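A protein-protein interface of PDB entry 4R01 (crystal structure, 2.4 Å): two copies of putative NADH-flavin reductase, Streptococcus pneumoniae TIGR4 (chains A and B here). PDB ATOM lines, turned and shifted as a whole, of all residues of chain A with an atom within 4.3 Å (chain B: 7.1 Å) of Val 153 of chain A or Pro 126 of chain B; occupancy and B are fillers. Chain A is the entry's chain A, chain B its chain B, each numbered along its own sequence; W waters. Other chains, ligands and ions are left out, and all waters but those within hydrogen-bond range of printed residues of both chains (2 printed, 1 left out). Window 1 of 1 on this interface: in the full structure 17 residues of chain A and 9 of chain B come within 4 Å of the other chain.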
ATOM      1  N   ALA A 101      10.516  -7.540  16.874  1.00  0.00           N
ATOM      2  CA  ALA A 101       9.668  -7.782  18.036  1.00  0.00           C
ATOM      3  C   ALA A 101       9.648  -9.261  18.407  1.00  0.00           C
ATOM      4  O   ALA A 101       9.304  -9.621  19.530  1.00  0.00           O
ATOM      5  CB  ALA A 101       8.252  -7.281  17.775  1.00  0.00           C
ATOM      6  N   PHE A 124       7.295 -15.393   8.972  1.00  0.00           N
ATOM      7  CA  PHE A 124       7.977 -14.358   9.739  1.00  0.00           C
ATOM      8  C   PHE A 124       9.251 -14.897  10.374  1.00  0.00           C
ATOM      9  O   PHE A 124      10.162 -14.138  10.707  1.00  0.00           O
ATOM     10  CB  PHE A 124       7.058 -13.788  10.825  1.00  0.00           C
ATOM     11  CG  PHE A 124       5.979 -12.882  10.300  1.00  0.00           C
ATOM     12  CD1 PHE A 124       5.814 -12.683   8.938  1.00  0.00           C
ATOM     13  CD2 PHE A 124       5.135 -12.219  11.177  1.00  0.00           C
ATOM     14  CE1 PHE A 124       4.823 -11.849   8.458  1.00  0.00           C
ATOM     15  CE2 PHE A 124       4.139 -11.383  10.704  1.00  0.00           C
ATOM     16  CZ  PHE A 124       3.985 -11.197   9.340  1.00  0.00           C
ATOM     17  N   PRO A 151      10.832  -2.953  17.901  1.00  0.00           N
ATOM     18  CA  PRO A 151       9.579  -2.272  17.581  1.00  0.00           C
ATOM     19  C   PRO A 151       8.401  -3.086  18.097  1.00  0.00           C
ATOM     20  O   PRO A 151       8.612  -4.116  18.742  1.00  0.00           O
ATOM     21  CB  PRO A 151       9.593  -2.225  16.054  1.00  0.00           C
ATOM     22  CG  PRO A 151      10.293  -3.494  15.676  1.00  0.00           C
ATOM     23  CD  PRO A 151      11.310  -3.771  16.774  1.00  0.00           C
ATOM     24  N   ALA A 152       7.182  -2.640  17.815  1.00  0.00           N
ATOM     25  CA  ALA A 152       6.001  -3.391  18.206  1.00  0.00           C
ATOM     26  C   ALA A 152       5.791  -4.560  17.252  1.00  0.00           C
ATOM     27  O   ALA A 152       6.496  -4.683  16.251  1.00  0.00           O
ATOM     28  CB  ALA A 152       4.784  -2.495  18.231  1.00  0.00           C
ATOM     29  N   VAL A 153       4.825  -5.417  17.569  1.00  0.00           N
ATOM     30  CA  VAL A 153       4.513  -6.565  16.727  1.00  0.00           C
ATOM     31  C   VAL A 153       4.111  -6.111  15.332  1.00  0.00           C
ATOM     32  O   VAL A 153       4.634  -6.601  14.330  1.00  0.00           O
ATOM     33  CB  VAL A 153       3.385  -7.414  17.335  1.00  0.00           C
ATOM     34  CG1 VAL A 153       2.946  -8.498  16.360  1.00  0.00           C
ATOM     35  CG2 VAL A 153       3.837  -8.013  18.657  1.00  0.00           C
ATOM     36  N   ASP A 154       3.184  -5.161  15.277  1.00  0.00           N
ATOM     37  CA  ASP A 154       2.770  -4.564  14.018  1.00  0.00           C
ATOM     38  C   ASP A 154       3.551  -3.271  13.789  1.00  0.00           C
ATOM     39  O   ASP A 154       3.274  -2.246  14.412  1.00  0.00           O
ATOM     40  CB  ASP A 154       1.263  -4.301  14.013  1.00  0.00           C
ATOM     41  CG  ASP A 154       0.721  -4.048  12.619  1.00  0.00           C
ATOM     42  OD1 ASP A 154       1.350  -4.501  11.638  1.00  0.00           O
ATOM     43  OD2 ASP A 154      -0.342  -3.405  12.503  1.00  0.00           O
ATOM     44  N   PHE A 155       4.523  -3.301  12.909  1.00  0.00           N
ATOM     45  CA  PHE A 155       5.408  -2.194  12.625  1.00  0.00           C
ATOM     46  C   PHE A 155       5.050  -1.632  11.263  1.00  0.00           C
ATOM     47  O   PHE A 155       5.204  -2.276  10.254  1.00  0.00           O
ATOM     48  CB  PHE A 155       6.833  -2.728  12.625  1.00  0.00           C
ATOM     49  CG  PHE A 155       7.895  -1.716  12.830  1.00  0.00           C
ATOM     50  CD1 PHE A 155       7.642  -0.520  13.433  1.00  0.00           C
ATOM     51  CD2 PHE A 155       9.156  -1.981  12.413  1.00  0.00           C
ATOM     52  CE1 PHE A 155       8.629   0.395  13.614  1.00  0.00           C
ATOM     53  CE2 PHE A 155      10.150  -1.082  12.600  1.00  0.00           C
ATOM     54  CZ  PHE A 155       9.889   0.108  13.204  1.00  0.00           C
ATOM     55  N   PHE A 172       7.457  -8.483  26.339  1.00  0.00           N
ATOM     56  CA  PHE A 172       6.348  -8.083  25.477  1.00  0.00           C
ATOM     57  C   PHE A 172       5.289  -7.283  26.235  1.00  0.00           C
ATOM     58  O   PHE A 172       4.829  -7.687  27.305  1.00  0.00           O
ATOM     59  CB  PHE A 172       5.710  -9.313  24.826  1.00  0.00           C
ATOM     60  CG  PHE A 172       4.440  -9.016  24.076  1.00  0.00           C
ATOM     61  CD1 PHE A 172       4.466  -8.265  22.913  1.00  0.00           C
ATOM     62  CD2 PHE A 172       3.224  -9.499  24.528  1.00  0.00           C
ATOM     63  CE1 PHE A 172       3.300  -7.996  22.222  1.00  0.00           C
ATOM     64  CE2 PHE A 172       2.058  -9.233  23.842  1.00  0.00           C
ATOM     65  CZ  PHE A 172       2.097  -8.480  22.687  1.00  0.00           C
ATOM     66  N   SER A 180      -0.350  -4.310  20.197  1.00  0.00           N
ATOM     67  CA  SER A 180       1.050  -3.949  20.027  1.00  0.00           C
ATOM     68  C   SER A 180       1.320  -3.495  18.595  1.00  0.00           C
ATOM     69  O   SER A 180       1.547  -4.318  17.707  1.00  0.00           O
ATOM     70  CB  SER A 180       1.958  -5.124  20.389  1.00  0.00           C
ATOM     71  OG  SER A 180       3.317  -4.804  20.151  1.00  0.00           O
ATOM     72  N   PRO B  71       8.034  -6.207   7.776  1.00  0.00           N
ATOM     73  CA  PRO B  71       7.447  -4.896   8.080  1.00  0.00           C
ATOM     74  C   PRO B  71       7.580  -3.897   6.925  1.00  0.00           C
ATOM     75  O   PRO B  71       6.644  -3.131   6.685  1.00  0.00           O
ATOM     76  CB  PRO B  71       8.248  -4.432   9.300  1.00  0.00           C
ATOM     77  CG  PRO B  71       8.645  -5.698   9.977  1.00  0.00           C
ATOM     78  CD  PRO B  71       8.889  -6.695   8.875  1.00  0.00           C
ATOM     79  N   LEU B  74       5.178  -5.630   3.842  1.00  0.00           N
ATOM     80  CA  LEU B  74       3.760  -5.906   4.090  1.00  0.00           C
ATOM     81  C   LEU B  74       2.795  -4.933   3.384  1.00  0.00           C
ATOM     82  O   LEU B  74       1.759  -5.368   2.881  1.00  0.00           O
ATOM     83  CB  LEU B  74       3.474  -5.917   5.599  1.00  0.00           C
ATOM     84  CG  LEU B  74       3.684  -7.249   6.323  1.00  0.00           C
ATOM     85  CD1 LEU B  74       3.604  -7.059   7.824  1.00  0.00           C
ATOM     86  CD2 LEU B  74       2.655  -8.267   5.869  1.00  0.00           C
ATOM     87  N   HIS B  77       0.980  -5.384  -0.395  1.00  0.00           N
ATOM     88  CA  HIS B  77      -0.305  -5.995  -0.714  1.00  0.00           C
ATOM     89  C   HIS B  77      -1.228  -4.954  -1.337  1.00  0.00           C
ATOM     90  O   HIS B  77      -1.805  -5.176  -2.403  1.00  0.00           O
ATOM     91  CB  HIS B  77      -0.958  -6.598   0.529  1.00  0.00           C
ATOM     92  CG  HIS B  77      -0.402  -7.933   0.919  1.00  0.00           C
ATOM     93  ND1 HIS B  77       0.544  -8.085   1.909  1.00  0.00           N
ATOM     94  CD2 HIS B  77      -0.666  -9.178   0.455  1.00  0.00           C
ATOM     95  CE1 HIS B  77       0.841  -9.367   2.039  1.00  0.00           C
ATOM     96  NE2 HIS B  77       0.118 -10.050   1.167  1.00  0.00           N
ATOM     97  N   PHE B 120      -8.580 -12.118  18.721  1.00  0.00           N
ATOM     98  CA  PHE B 120      -7.769 -12.309  17.524  1.00  0.00           C
ATOM     99  C   PHE B 120      -6.289 -12.184  17.888  1.00  0.00           C
ATOM    100  O   PHE B 120      -5.858 -11.159  18.416  1.00  0.00           O
ATOM    101  CB  PHE B 120      -8.143 -11.307  16.430  1.00  0.00           C
ATOM    102  CG  PHE B 120      -7.493 -11.595  15.103  1.00  0.00           C
ATOM    103  CD1 PHE B 120      -8.106 -12.434  14.182  1.00  0.00           C
ATOM    104  CD2 PHE B 120      -6.262 -11.039  14.781  1.00  0.00           C
ATOM    105  CE1 PHE B 120      -7.507 -12.705  12.964  1.00  0.00           C
ATOM    106  CE2 PHE B 120      -5.662 -11.306  13.569  1.00  0.00           C
ATOM    107  CZ  PHE B 120      -6.285 -12.142  12.658  1.00  0.00           C
ATOM    108  N   PRO B 121      -5.512 -13.240  17.613  1.00  0.00           N
ATOM    109  CA  PRO B 121      -4.108 -13.327  18.031  1.00  0.00           C
ATOM    110  C   PRO B 121      -3.265 -12.179  17.489  1.00  0.00           C
ATOM    111  O   PRO B 121      -3.332 -11.857  16.304  1.00  0.00           O
ATOM    112  CB  PRO B 121      -3.647 -14.677  17.465  1.00  0.00           C
ATOM    113  CG  PRO B 121      -4.657 -15.044  16.448  1.00  0.00           C
ATOM    114  CD  PRO B 121      -5.943 -14.432  16.867  1.00  0.00           C
ATOM    115  N   GLU B 122      -2.488 -11.568  18.377  1.00  0.00           N
ATOM    116  CA  GLU B 122      -1.726 -10.369  18.059  1.00  0.00           C
ATOM    117  C   GLU B 122      -0.707 -10.609  16.950  1.00  0.00           C
ATOM    118  O   GLU B 122      -0.477  -9.738  16.114  1.00  0.00           O
ATOM    119  CB  GLU B 122      -1.022  -9.849  19.316  1.00  0.00           C
ATOM    120  CG  GLU B 122      -0.503  -8.426  19.201  1.00  0.00           C
ATOM    121  CD  GLU B 122      -1.618  -7.396  19.157  1.00  0.00           C
ATOM    122  OE1 GLU B 122      -2.761  -7.726  19.545  1.00  0.00           O
ATOM    123  OE2 GLU B 122      -1.351  -6.251  18.736  1.00  0.00           O
ATOM    124  N   GLU B 123      -0.109 -11.797  16.945  1.00  0.00           N
ATOM    125  CA  GLU B 123       0.914 -12.143  15.963  1.00  0.00           C
ATOM    126  C   GLU B 123       0.352 -12.302  14.548  1.00  0.00           C
ATOM    127  O   GLU B 123       1.106 -12.286  13.574  1.00  0.00           O
ATOM    128  CB  GLU B 123       1.634 -13.432  16.376  1.00  0.00           C
ATOM    129  CG  GLU B 123       2.634 -13.266  17.516  1.00  0.00           C
ATOM    130  CD  GLU B 123       3.871 -12.477  17.113  1.00  0.00           C
ATOM    131  OE1 GLU B 123       4.090 -12.274  15.899  1.00  0.00           O
ATOM    132  OE2 GLU B 123       4.631 -12.065  18.014  1.00  0.00           O
ATOM    133  N   PHE B 124      -0.965 -12.459  14.432  1.00  0.00           N
ATOM    134  CA  PHE B 124      -1.597 -12.601  13.121  1.00  0.00           C
ATOM    135  C   PHE B 124      -1.987 -11.248  12.537  1.00  0.00           C
ATOM    136  O   PHE B 124      -2.349 -11.151  11.366  1.00  0.00           O
ATOM    137  CB  PHE B 124      -2.842 -13.492  13.200  1.00  0.00           C
ATOM    138  CG  PHE B 124      -2.542 -14.957  13.354  1.00  0.00           C
ATOM    139  CD1 PHE B 124      -1.238 -15.415  13.433  1.00  0.00           C
ATOM    140  CD2 PHE B 124      -3.574 -15.883  13.400  1.00  0.00           C
ATOM    141  CE1 PHE B 124      -0.971 -16.763  13.572  1.00  0.00           C
ATOM    142  CE2 PHE B 124      -3.313 -17.230  13.542  1.00  0.00           C
ATOM    143  CZ  PHE B 124      -2.009 -17.671  13.626  1.00  0.00           C
ATOM    144  N   LYS B 125      -1.913 -10.208  13.358  1.00  0.00           N
ATOM    145  CA  LYS B 125      -2.401  -8.890  12.958  1.00  0.00           C
ATOM    146  C   LYS B 125      -1.575  -8.174  11.869  1.00  0.00           C
ATOM    147  O   LYS B 125      -2.161  -7.520  11.008  1.00  0.00           O
ATOM    148  CB  LYS B 125      -2.524  -7.994  14.192  1.00  0.00           C
ATOM    149  CG  LYS B 125      -3.623  -8.444  15.137  1.00  0.00           C
ATOM    150  CD  LYS B 125      -3.816  -7.479  16.287  1.00  0.00           C
ATOM    151  CE  LYS B 125      -4.996  -7.894  17.150  1.00  0.00           C
ATOM    152  NZ  LYS B 125      -5.139  -7.014  18.343  1.00  0.00           N
ATOM    153  N   PRO B 126      -0.230  -8.272  11.902  1.00  0.00           N
ATOM    154  CA  PRO B 126       0.517  -7.656  10.795  1.00  0.00           C
ATOM    155  C   PRO B 126       0.024  -8.075   9.408  1.00  0.00           C
ATOM    156  O   PRO B 126      -0.289  -7.213   8.586  1.00  0.00           O
ATOM    157  CB  PRO B 126       1.945  -8.145  11.032  1.00  0.00           C
ATOM    158  CG  PRO B 126       2.038  -8.255  12.511  1.00  0.00           C
ATOM    159  CD  PRO B 126       0.678  -8.723  12.978  1.00  0.00           C
ATOM    160  N   LEU B 127      -0.069  -9.377   9.163  1.00  0.00           N
ATOM    161  CA  LEU B 127      -0.523  -9.867   7.866  1.00  0.00           C
ATOM    162  C   LEU B 127      -2.022  -9.649   7.646  1.00  0.00           C
ATOM    163  O   LEU B 127      -2.447  -9.300   6.545  1.00  0.00           O
ATOM    164  CB  LEU B 127      -0.183 -11.350   7.713  1.00  0.00           C
ATOM    165  CG  LEU B 127      -0.625 -12.019   6.411  1.00  0.00           C
ATOM    166  CD1 LEU B 127      -0.132 -11.236   5.202  1.00  0.00           C
ATOM    167  CD2 LEU B 127      -0.122 -13.452   6.359  1.00  0.00           C
ATOM    168  N   ALA B 128      -2.819  -9.856   8.691  1.00  0.00           N
ATOM    169  CA  ALA B 128      -4.269  -9.726   8.576  1.00  0.00           C
ATOM    170  C   ALA B 128      -4.684  -8.302   8.216  1.00  0.00           C
ATOM    171  O   ALA B 128      -5.538  -8.093   7.351  1.00  0.00           O
ATOM    172  CB  ALA B 128      -4.944 -10.159   9.869  1.00  0.00           C
ATOM    173  N   LYS B 129      -4.082  -7.325   8.887  1.00  0.00           N
ATOM    174  CA  LYS B 129      -4.391  -5.925   8.629  1.00  0.00           C
ATOM    175  C   LYS B 129      -3.928  -5.509   7.236  1.00  0.00           C
ATOM    176  O   LYS B 129      -4.615  -4.749   6.549  1.00  0.00           O
ATOM    177  CB  LYS B 129      -3.755  -5.027   9.693  1.00  0.00           C
ATOM    178  CG  LYS B 129      -4.437  -5.104  11.052  1.00  0.00           C
ATOM    179  CD  LYS B 129      -3.707  -4.264  12.088  1.00  0.00           C
ATOM    180  CE  LYS B 129      -3.592  -2.815  11.644  1.00  0.00           C
ATOM    181  NZ  LYS B 129      -2.764  -2.016  12.588  1.00  0.00           N
ATOM    182  N   ALA B 130      -2.768  -6.012   6.824  1.00  0.00           N
ATOM    183  CA  ALA B 130      -2.246  -5.733   5.489  1.00  0.00           C
ATOM    184  C   ALA B 130      -3.216  -6.228   4.421  1.00  0.00           C
ATOM    185  O   ALA B 130      -3.525  -5.512   3.469  1.00  0.00           O
ATOM    186  CB  ALA B 130      -0.876  -6.373   5.303  1.00  0.00           C
ATOM    187  N   GLN B 131      -3.697  -7.455   4.592  1.00  0.00           N
ATOM    188  CA  GLN B 131      -4.664  -8.033   3.669  1.00  0.00           C
ATOM    189  C   GLN B 131      -6.024  -7.355   3.777  1.00  0.00           C
ATOM    190  O   GLN B 131      -6.787  -7.333   2.814  1.00  0.00           O
ATOM    191  CB  GLN B 131      -4.810  -9.533   3.914  1.00  0.00           C
ATOM    192  CG  GLN B 131      -3.585 -10.339   3.524  1.00  0.00           C
ATOM    193  CD  GLN B 131      -3.696 -11.793   3.936  1.00  0.00           C
ATOM    194  OE1 GLN B 131      -4.031 -12.104   5.083  1.00  0.00           O
ATOM    195  NE2 GLN B 131      -3.425 -12.692   3.000  1.00  0.00           N
ATOM    196  N   ALA B 132      -6.322  -6.798   4.948  1.00  0.00           N
ATOM    197  CA  ALA B 132      -7.575  -6.078   5.155  1.00  0.00           C
ATOM    198  C   ALA B 132      -7.544  -4.715   4.468  1.00  0.00           C
ATOM    199  O   ALA B 132      -8.539  -4.283   3.890  1.00  0.00           O
ATOM    200  CB  ALA B 132      -7.863  -5.916   6.642  1.00  0.00           C
ATOM    201  N   ASP B 133      -6.400  -4.037   4.538  1.00  0.00           N
ATOM    202  CA  ASP B 133      -6.218  -2.772   3.831  1.00  0.00           C
ATOM    203  C   ASP B 133      -6.276  -3.011   2.329  1.00  0.00           C
ATOM    204  O   ASP B 133      -6.689  -2.147   1.558  1.00  0.00           O
ATOM    205  CB  ASP B 133      -4.887  -2.116   4.204  1.00  0.00           C
ATOM    206  CG  ASP B 133      -4.782  -1.807   5.683  1.00  0.00           C
ATOM    207  OD1 ASP B 133      -5.835  -1.659   6.341  1.00  0.00           O
ATOM    208  OD2 ASP B 133      -3.643  -1.710   6.185  1.00  0.00           O
HETATM  209  O   HOH W   1      -0.558  -5.761  16.358  1.00  0.00           O
HETATM  210  O   HOH W   2       0.317  -4.469   8.953  1.00  0.00           O
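NZ of Lys 129 of chain B is in salt-bridge range of OD2 of Asp 154 of chain A. The backbone NH (N) of Ser 180 of chain A lies within hydrogen-bond range of the side-chain carboxylate (OE2) of Glu 122 of chain B (2.6 Å).
The side-chain amino group of Lys 125 of chain B lies within salt-bridge range of the side-chain carboxylate of Glu 122 of chain B (2.8 Å). The side-chain hydroxyl (OG) of Ser 180 of chain A lies within hydrogen-bond range of the backbone NH (N) of Val 153 of chain A (3.1 Å). N of Asp 154 of chain A sits at hydrogen-bond distance from O of Ser 180 of chain A (3.0 Å).
CE2 of Phe 124 of chain A touches CB of Pro 126 of chain B (3.9 Å). Glu 122 of chain B touches Val 153 of chain A. CG1 of Val 153 of chain A touches OE1 of Glu 123 of chain B, at 3.97 Å. O of Val 153 of chain A touches CG of Pro 126 of chain B, at 3.6 Å. Asp 154 of chain A touches Pro 126 of chain B. Pro 71 of chain B touches Phe 155 of chain A (CB to O, 3.9 Å).
Val 153 of chain A touches just these residues of chain B: Glu 122 (3.6 Å), Glu 123 (3.97 Å) and Pro 126 (3.6 Å). Of the printed residues of chain B, Phe 155 of chain A touches Pro 71 (3.9 Å). Of the printed residues of chain B, Ser 180 of chain A touches Glu 122 (2.6 Å). Pro 151 of chain A touches none of the printed residues of chain B. The nearest printed residue of chain B that does not touch Val 153 of chain A is Phe 124 of chain B (5.9 Å). The nearest printed residue of chain A that does not touch Pro 126 of chain B is Phe 155 of chain A (5.6 Å).
Printed residues of chain A that touch a printed residue of chain B: Phe 124, Val 153, Asp 154, Phe 155 and Ser 180. Hydrophobic or aromatic side chains of chain A that line the printed part of chain B: Phe 124, Val 153 and Phe 155. Of the 17 printed residues of chain B, 5 touch a printed residue of chain A. Hydrophobic or aromatic side chains of chain B that line the printed part of chain A: Pro 71 and Pro 126. Among the printed residues, 8 pairs touch across the chains.
1 position is printed for both chains. Of the 8 pairs that touch across the chains among the printed residues, none has its exchanged pair printed and touching as well.
Water W1 bridges the side-chain carboxylate of Glu 122 of chain B and the backbone carbonyl oxygen of Ser 180 of chain A. Water W2 lies within hydrogen-bond range of O of Pro 126 of chain B and OD1 of Asp 154 of chain A.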
